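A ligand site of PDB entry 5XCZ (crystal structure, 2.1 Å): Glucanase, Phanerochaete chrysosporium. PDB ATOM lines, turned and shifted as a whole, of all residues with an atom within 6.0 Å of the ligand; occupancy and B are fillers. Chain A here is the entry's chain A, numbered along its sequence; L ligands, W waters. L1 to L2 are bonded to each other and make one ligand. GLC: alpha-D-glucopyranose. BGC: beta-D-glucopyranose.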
ATOM      1  N   TYR A  83     -11.222  -5.522  18.305  1.00  0.00           N
ATOM      2  CA  TYR A  83     -12.554  -4.907  18.514  1.00  0.00           C
ATOM      3  C   TYR A  83     -12.413  -3.392  18.679  1.00  0.00           C
ATOM      4  O   TYR A  83     -12.596  -2.830  19.765  1.00  0.00           O
ATOM      5  CB  TYR A  83     -13.272  -5.495  19.726  1.00  0.00           C
ATOM      6  CG  TYR A  83     -14.711  -5.053  19.908  1.00  0.00           C
ATOM      7  CD1 TYR A  83     -15.680  -5.342  18.944  1.00  0.00           C
ATOM      8  CD2 TYR A  83     -15.109  -4.365  21.058  1.00  0.00           C
ATOM      9  CE1 TYR A  83     -17.022  -4.955  19.116  1.00  0.00           C
ATOM     10  CE2 TYR A  83     -16.433  -3.973  21.247  1.00  0.00           C
ATOM     11  CZ  TYR A  83     -17.382  -4.282  20.271  1.00  0.00           C
ATOM     12  OH  TYR A  83     -18.692  -3.889  20.457  1.00  0.00           O
ATOM     13  N   ASP A  89     -20.036  -1.030  16.620  1.00  0.00           N
ATOM     14  CA  ASP A  89     -21.386  -1.283  17.133  1.00  0.00           C
ATOM     15  C   ASP A  89     -22.430  -0.450  16.381  1.00  0.00           C
ATOM     16  O   ASP A  89     -23.128   0.368  16.943  1.00  0.00           O
ATOM     17  CB  ASP A  89     -21.431  -1.018  18.647  1.00  0.00           C
ATOM     18  CG  ASP A  89     -22.389  -1.969  19.412  1.00  0.00           C
ATOM     19  OD1 ASP A  89     -22.712  -3.073  18.903  1.00  0.00           O
ATOM     20  OD2 ASP A  89     -22.822  -1.603  20.533  1.00  0.00           O
ATOM     21  N   ALA A  91     -25.306  -1.050  14.996  1.00  0.00           N
ATOM     22  CA  ALA A  91     -26.751  -1.195  15.132  1.00  0.00           C
ATOM     23  C   ALA A  91     -27.221  -1.110  16.578  1.00  0.00           C
ATOM     24  O   ALA A  91     -28.388  -1.355  16.860  1.00  0.00           O
ATOM     25  CB  ALA A  91     -27.218  -2.511  14.497  1.00  0.00           C
ATOM     26  N   ALA A  92     -26.324  -0.748  17.505  1.00  0.00           N
ATOM     27  CA  ALA A  92     -26.655  -0.503  18.891  1.00  0.00           C
ATOM     28  C   ALA A  92     -25.923   0.742  19.341  1.00  0.00           C
ATOM     29  O   ALA A  92     -25.215   1.375  18.557  1.00  0.00           O
ATOM     30  CB  ALA A  92     -26.284  -1.708  19.766  1.00  0.00           C
ATOM     31  N   ALA A  94     -24.582   0.693  22.937  1.00  0.00           N
ATOM     32  CA  ALA A  94     -23.903   0.411  24.204  1.00  0.00           C
ATOM     33  C   ALA A  94     -22.388   0.327  24.058  1.00  0.00           C
ATOM     34  O   ALA A  94     -21.653   0.712  24.982  1.00  0.00           O
ATOM     35  CB  ALA A  94     -24.443  -0.884  24.805  1.00  0.00           C
ATOM     36  N   SER A  95     -21.880  -0.167  22.931  1.00  0.00           N
ATOM     37  CA  SER A  95     -20.449  -0.403  22.802  1.00  0.00           C
ATOM     38  C   SER A  95     -19.809   0.458  21.720  1.00  0.00           C
ATOM     39  O   SER A  95     -18.818   0.047  21.105  1.00  0.00           O
ATOM     40  CB  SER A  95     -20.182  -1.883  22.522  1.00  0.00           C
ATOM     41  OG  SER A  95     -18.920  -2.272  23.055  1.00  0.00           O
ATOM     42  N   ASP A 135     -19.492  -8.601  15.882  1.00  0.00           N
ATOM     43  CA  ASP A 135     -20.732  -7.955  15.432  1.00  0.00           C
ATOM     44  C   ASP A 135     -20.641  -7.325  14.047  1.00  0.00           C
ATOM     45  O   ASP A 135     -21.666  -7.093  13.399  1.00  0.00           O
ATOM     46  CB  ASP A 135     -21.198  -6.925  16.442  1.00  0.00           C
ATOM     47  CG  ASP A 135     -21.510  -7.537  17.784  1.00  0.00           C
ATOM     48  OD1 ASP A 135     -21.801  -8.762  17.833  1.00  0.00           O
ATOM     49  OD2 ASP A 135     -21.440  -6.816  18.798  1.00  0.00           O
ATOM     50  N   ASN A 139     -23.639  -7.520  11.270  1.00  0.00           N
ATOM     51  CA  ASN A 139     -24.387  -6.304  10.961  1.00  0.00           C
ATOM     52  C   ASN A 139     -24.486  -6.084   9.456  1.00  0.00           C
ATOM     53  O   ASN A 139     -25.515  -5.619   8.960  1.00  0.00           O
ATOM     54  CB  ASN A 139     -23.745  -5.097  11.660  1.00  0.00           C
ATOM     55  CG  ASN A 139     -24.232  -4.966  13.082  1.00  0.00           C
ATOM     56  OD1 ASN A 139     -25.419  -5.172  13.352  1.00  0.00           O
ATOM     57  ND2 ASN A 139     -23.322  -4.652  14.013  1.00  0.00           N
ATOM     58  N   THR A 142     -27.537  -8.456   8.053  1.00  0.00           N
ATOM     59  CA  THR A 142     -28.924  -8.218   8.390  1.00  0.00           C
ATOM     60  C   THR A 142     -29.278  -6.764   8.659  1.00  0.00           C
ATOM     61  O   THR A 142     -30.464  -6.457   8.844  1.00  0.00           O
ATOM     62  CB  THR A 142     -29.326  -9.024   9.633  1.00  0.00           C
ATOM     63  OG1 THR A 142     -28.732  -8.405  10.787  1.00  0.00           O
ATOM     64  CG2 THR A 142     -28.828 -10.428   9.524  1.00  0.00           C
ATOM     65  N   ASN A 143     -28.296  -5.859   8.729  1.00  0.00           N
ATOM     66  CA  ASN A 143     -28.534  -4.503   9.196  1.00  0.00           C
ATOM     67  C   ASN A 143     -28.073  -3.455   8.174  1.00  0.00           C
ATOM     68  O   ASN A 143     -27.663  -2.358   8.543  1.00  0.00           O
ATOM     69  CB  ASN A 143     -27.857  -4.273  10.544  1.00  0.00           C
ATOM     70  CG  ASN A 143     -28.647  -4.868  11.719  1.00  0.00           C
ATOM     71  OD1 ASN A 143     -29.874  -4.786  11.749  1.00  0.00           O
ATOM     72  ND2 ASN A 143     -27.950  -5.448  12.697  1.00  0.00           N
ATOM     73  N   HIS A 180     -24.449 -15.316  15.918  1.00  0.00           N
ATOM     74  CA  HIS A 180     -24.937 -16.454  16.702  1.00  0.00           C
ATOM     75  C   HIS A 180     -26.197 -16.997  16.046  1.00  0.00           C
ATOM     76  O   HIS A 180     -26.671 -16.458  15.042  1.00  0.00           O
ATOM     77  CB  HIS A 180     -25.195 -16.063  18.156  1.00  0.00           C
ATOM     78  CG  HIS A 180     -26.253 -15.016  18.342  1.00  0.00           C
ATOM     79  ND1 HIS A 180     -27.589 -15.326  18.439  1.00  0.00           N
ATOM     80  CD2 HIS A 180     -26.164 -13.672  18.460  1.00  0.00           C
ATOM     81  CE1 HIS A 180     -28.286 -14.218  18.609  1.00  0.00           C
ATOM     82  NE2 HIS A 180     -27.448 -13.199  18.629  1.00  0.00           N
ATOM     83  N   GLY A 182     -29.426 -17.095  16.756  1.00  0.00           N
ATOM     84  CA  GLY A 182     -30.566 -16.210  16.581  1.00  0.00           C
ATOM     85  C   GLY A 182     -30.335 -15.026  15.665  1.00  0.00           C
ATOM     86  O   GLY A 182     -31.282 -14.302  15.332  1.00  0.00           O
ATOM     87  N   TRP A 183     -29.087 -14.825  15.231  1.00  0.00           N
ATOM     88  CA  TRP A 183     -28.752 -13.735  14.319  1.00  0.00           C
ATOM     89  C   TRP A 183     -28.644 -14.296  12.908  1.00  0.00           C
ATOM     90  O   TRP A 183     -29.602 -14.224  12.126  1.00  0.00           O
ATOM     91  CB  TRP A 183     -27.447 -13.036  14.737  1.00  0.00           C
ATOM     92  CG  TRP A 183     -27.266 -11.644  14.161  1.00  0.00           C
ATOM     93  CD1 TRP A 183     -27.940 -11.091  13.111  1.00  0.00           C
ATOM     94  CD2 TRP A 183     -26.341 -10.636  14.598  1.00  0.00           C
ATOM     95  NE1 TRP A 183     -27.505  -9.814  12.873  1.00  0.00           N
ATOM     96  CE2 TRP A 183     -26.514  -9.510  13.769  1.00  0.00           C
ATOM     97  CE3 TRP A 183     -25.375 -10.578  15.617  1.00  0.00           C
ATOM     98  CZ2 TRP A 183     -25.772  -8.336  13.919  1.00  0.00           C
ATOM     99  CZ3 TRP A 183     -24.639  -9.411  15.769  1.00  0.00           C
ATOM    100  CH2 TRP A 183     -24.842  -8.304  14.928  1.00  0.00           C
ATOM    101  N   VAL A 217     -20.360 -14.984  20.533  1.00  0.00           N
ATOM    102  CA  VAL A 217     -19.516 -14.107  21.323  1.00  0.00           C
ATOM    103  C   VAL A 217     -20.379 -13.093  22.053  1.00  0.00           C
ATOM    104  O   VAL A 217     -21.194 -12.374  21.448  1.00  0.00           O
ATOM    105  CB  VAL A 217     -18.481 -13.399  20.435  1.00  0.00           C
ATOM    106  CG1 VAL A 217     -17.764 -12.299  21.238  1.00  0.00           C
ATOM    107  CG2 VAL A 217     -17.477 -14.412  19.863  1.00  0.00           C
ATOM    108  N   ALA A 218     -20.193 -13.018  23.374  1.00  0.00           N
ATOM    109  CA  ALA A 218     -20.913 -12.094  24.233  1.00  0.00           C
ATOM    110  C   ALA A 218     -22.413 -12.357  24.222  1.00  0.00           C
ATOM    111  O   ALA A 218     -23.203 -11.491  24.609  1.00  0.00           O
ATOM    112  CB  ALA A 218     -20.645 -10.630  23.867  1.00  0.00           C
ATOM    113  N   ASN A 219     -22.826 -13.529  23.772  1.00  0.00           N
ATOM    114  CA  ASN A 219     -24.236 -13.894  23.839  1.00  0.00           C
ATOM    115  C   ASN A 219     -24.377 -15.069  24.808  1.00  0.00           C
ATOM    116  O   ASN A 219     -23.465 -15.354  25.589  1.00  0.00           O
ATOM    117  CB  ASN A 219     -24.802 -14.189  22.438  1.00  0.00           C
ATOM    118  CG  ASN A 219     -26.299 -13.888  22.344  1.00  0.00           C
ATOM    119  OD1 ASN A 219     -27.142 -14.658  22.834  1.00  0.00           O
ATOM    120  ND2 ASN A 219     -26.628 -12.736  21.757  1.00  0.00           N
ATOM    121  N   TRP A 276     -35.155 -13.129  21.958  1.00  0.00           N
ATOM    122  CA  TRP A 276     -33.801 -13.561  21.584  1.00  0.00           C
ATOM    123  C   TRP A 276     -32.857 -12.369  21.456  1.00  0.00           C
ATOM    124  O   TRP A 276     -31.708 -12.431  21.902  1.00  0.00           O
ATOM    125  CB  TRP A 276     -33.842 -14.363  20.289  1.00  0.00           C
ATOM    126  CG  TRP A 276     -32.808 -15.463  20.207  1.00  0.00           C
ATOM    127  CD1 TRP A 276     -31.666 -15.595  20.973  1.00  0.00           C
ATOM    128  CD2 TRP A 276     -32.818 -16.578  19.311  1.00  0.00           C
ATOM    129  NE1 TRP A 276     -30.991 -16.744  20.608  1.00  0.00           N
ATOM    130  CE2 TRP A 276     -31.673 -17.356  19.594  1.00  0.00           C
ATOM    131  CE3 TRP A 276     -33.688 -17.011  18.307  1.00  0.00           C
ATOM    132  CZ2 TRP A 276     -31.377 -18.526  18.893  1.00  0.00           C
ATOM    133  CZ3 TRP A 276     -33.392 -18.165  17.615  1.00  0.00           C
ATOM    134  CH2 TRP A 276     -32.246 -18.912  17.913  1.00  0.00           C
ATOM    135  N   GLY A 277     -33.331 -11.269  20.874  1.00  0.00           N
ATOM    136  CA  GLY A 277     -32.514 -10.085  20.689  1.00  0.00           C
ATOM    137  C   GLY A 277     -32.125  -9.346  21.957  1.00  0.00           C
ATOM    138  O   GLY A 277     -31.454  -8.317  21.874  1.00  0.00           O
ATOM    139  N   ASP A 278     -32.525  -9.845  23.135  1.00  0.00           N
ATOM    140  CA  ASP A 278     -32.124  -9.235  24.400  1.00  0.00           C
ATOM    141  C   ASP A 278     -30.710  -9.704  24.719  1.00  0.00           C
ATOM    142  O   ASP A 278     -30.499 -10.817  25.210  1.00  0.00           O
ATOM    143  CB  ASP A 278     -33.084  -9.620  25.515  1.00  0.00           C
ATOM    144  CG  ASP A 278     -34.519  -9.212  25.239  1.00  0.00           C
ATOM    145  OD1 ASP A 278     -34.766  -8.447  24.281  1.00  0.00           O
ATOM    146  OD2 ASP A 278     -35.409  -9.653  26.000  1.00  0.00           O
ATOM    147  N   TRP A 279     -29.709  -8.842  24.473  1.00  0.00           N
ATOM    148  CA  TRP A 279     -28.319  -9.229  24.611  1.00  0.00           C
ATOM    149  C   TRP A 279     -27.594  -8.579  25.776  1.00  0.00           C
ATOM    150  O   TRP A 279     -26.448  -8.943  26.039  1.00  0.00           O
ATOM    151  CB  TRP A 279     -27.564  -8.904  23.317  1.00  0.00           C
ATOM    152  CG  TRP A 279     -27.846  -7.544  22.805  1.00  0.00           C
ATOM    153  CD1 TRP A 279     -28.763  -7.201  21.852  1.00  0.00           C
ATOM    154  CD2 TRP A 279     -27.208  -6.315  23.213  1.00  0.00           C
ATOM    155  NE1 TRP A 279     -28.738  -5.826  21.638  1.00  0.00           N
ATOM    156  CE2 TRP A 279     -27.792  -5.270  22.465  1.00  0.00           C
ATOM    157  CE3 TRP A 279     -26.201  -5.992  24.124  1.00  0.00           C
ATOM    158  CZ2 TRP A 279     -27.393  -3.929  22.605  1.00  0.00           C
ATOM    159  CZ3 TRP A 279     -25.801  -4.666  24.267  1.00  0.00           C
ATOM    160  CH2 TRP A 279     -26.405  -3.661  23.507  1.00  0.00           C
HETATM  161  C1  GLC L   1     -30.706  -9.828  16.887  1.00  0.00           C
HETATM  162  C2  GLC L   1     -29.617 -10.606  17.634  1.00  0.00           C
HETATM  163  C3  GLC L   1     -28.724  -9.635  18.390  1.00  0.00           C
HETATM  164  C4  GLC L   1     -28.243  -8.480  17.513  1.00  0.00           C
HETATM  165  C5  GLC L   1     -29.334  -7.926  16.584  1.00  0.00           C
HETATM  166  C6  GLC L   1     -28.695  -6.993  15.564  1.00  0.00           C
HETATM  167  O1  GLC L   1     -31.396  -8.985  17.814  1.00  0.00           O
HETATM  168  O2  GLC L   1     -30.173 -11.555  18.557  1.00  0.00           O
HETATM  169  O3  GLC L   1     -27.591 -10.379  18.845  1.00  0.00           O
HETATM  170  O4  GLC L   1     -27.842  -7.391  18.358  1.00  0.00           O
HETATM  171  O5  GLC L   1     -30.058  -8.985  15.941  1.00  0.00           O
HETATM  172  O6  GLC L   1     -29.639  -6.006  15.151  1.00  0.00           O
HETATM  173  C2  BGC L   2     -25.918  -6.038  19.015  1.00  0.00           C
HETATM  174  C3  BGC L   2     -24.531  -6.009  19.566  1.00  0.00           C
HETATM  175  C4  BGC L   2     -24.243  -7.143  20.456  1.00  0.00           C
HETATM  176  C5  BGC L   2     -24.551  -8.458  19.852  1.00  0.00           C
HETATM  177  C6  BGC L   2     -24.194  -9.534  20.855  1.00  0.00           C
HETATM  178  C1  BGC L   2     -26.421  -7.430  18.553  1.00  0.00           C
HETATM  179  O2  BGC L   2     -26.024  -5.122  17.926  1.00  0.00           O
HETATM  180  O3  BGC L   2     -24.400  -4.734  20.313  1.00  0.00           O
HETATM  181  O4  BGC L   2     -22.841  -7.197  20.903  1.00  0.00           O
HETATM  182  O5  BGC L   2     -25.989  -8.537  19.524  1.00  0.00           O
HETATM  183  O6  BGC L   2     -24.919 -10.723  20.570  1.00  0.00           O
HETATM  184  O   HOH W   1     -19.599  -7.870  21.208  1.00  0.00           O
HETATM  185  O   HOH W   2     -28.843  -4.238  17.478  1.00  0.00           O
HETATM  186  O   HOH W   3     -24.490  -3.323  16.742  1.00  0.00           O
HETATM  187  O   HOH W   4     -31.760  -6.677  19.855  1.00  0.00           O
HETATM  188  O   HOH W   5     -22.978  -3.714  22.072  1.00  0.00           O
HETATM  189  O   HOH W   6     -23.015 -12.222  19.329  1.00  0.00           O
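O of Asp 135 lies within hydrogen-bond range of ND2 of Asn 139 (3.0 Å).
The backbone NH (N) of Ser 95 lies within hydrogen-bond range of the side-chain carboxylate (OD2) of Asp 89, 2.9 Å away.
The side-chain amide nitrogen (ND2) of Asn 219 is in hydrogen-bond range of a ring nitrogen (NE2) of His 180, 3.3 Å away.
The backbone NH (N) of Gly 182 lies within hydrogen-bond range of a ring nitrogen (ND1) of His 180, 3.1 Å away.
The side-chain amide oxygen (OD1) of Asn 139 lies within hydrogen-bond range of the side-chain amide nitrogen (ND2) of Asn 143, at 2.6 Å.
The indole nitrogen (NE1) of Trp 183 is in hydrogen-bond range of the side-chain hydroxyl (OG1) of Thr 142, at 2.8 Å.
Merely in contact with the ligand: Ala 92 (3.6 Å), Trp 183 (3.6 Å), Trp 276 (3.8 Å), Gly 277 (3.3 Å) and Trp 279 (3.6 Å).
Hydrophobic or aromatic side chains within 4 Å of the ligand: Ala 92, His 180, Trp 183 and Trp 279.
Within 4 Å of the ligand: Asp 89, Ala 92, Asp 135, Asn 143, His 180, Trp 183, Asn 219, Trp 276, Gly 277 and Trp 279.
The nearest printed residue that does not touch the ligand is Val 217 (4.2 Å).
Water W5 lies within hydrogen-bond range of O3 of BGC L2 and OD2 of Asp 89.
Water W6 bridges O6 of BGC L2 (2.7 Å) and O of Val 217 (2.8 Å).
Water W2 bridges the backbone carbonyl oxygen (O) of Ala 91 and an oxygen (O2) of BGC L2.
Water W4 bridges the backbone carbonyl oxygen (O) of Gly 277 (2.6 Å) and an oxygen (O1) of GLC L1 (3.1 Å).
Water W1 lies within hydrogen-bond range of OD2 of Asp 135 and O4 of BGC L2.
O4 of BGC L2 lies within hydrogen-bond range of OD2 of Asp 135 (2.6 Å).
The side-chain carboxylate (OD1) of Asp 89 sits at hydrogen-bond distance from an oxygen (O3) of BGC L2 (2.8 Å).
O3 of GLC L1 sits at hydrogen-bond distance from NE2 of His 180, 2.8 Å away.
O6 of BGC L2 sits at hydrogen-bond distance from ND2 of Asn 219, 2.9 Å away.
The side-chain amide nitrogen (ND2) of Asn 143 is in hydrogen-bond range of an oxygen (O6) of GLC L1, 3.0 Å away.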
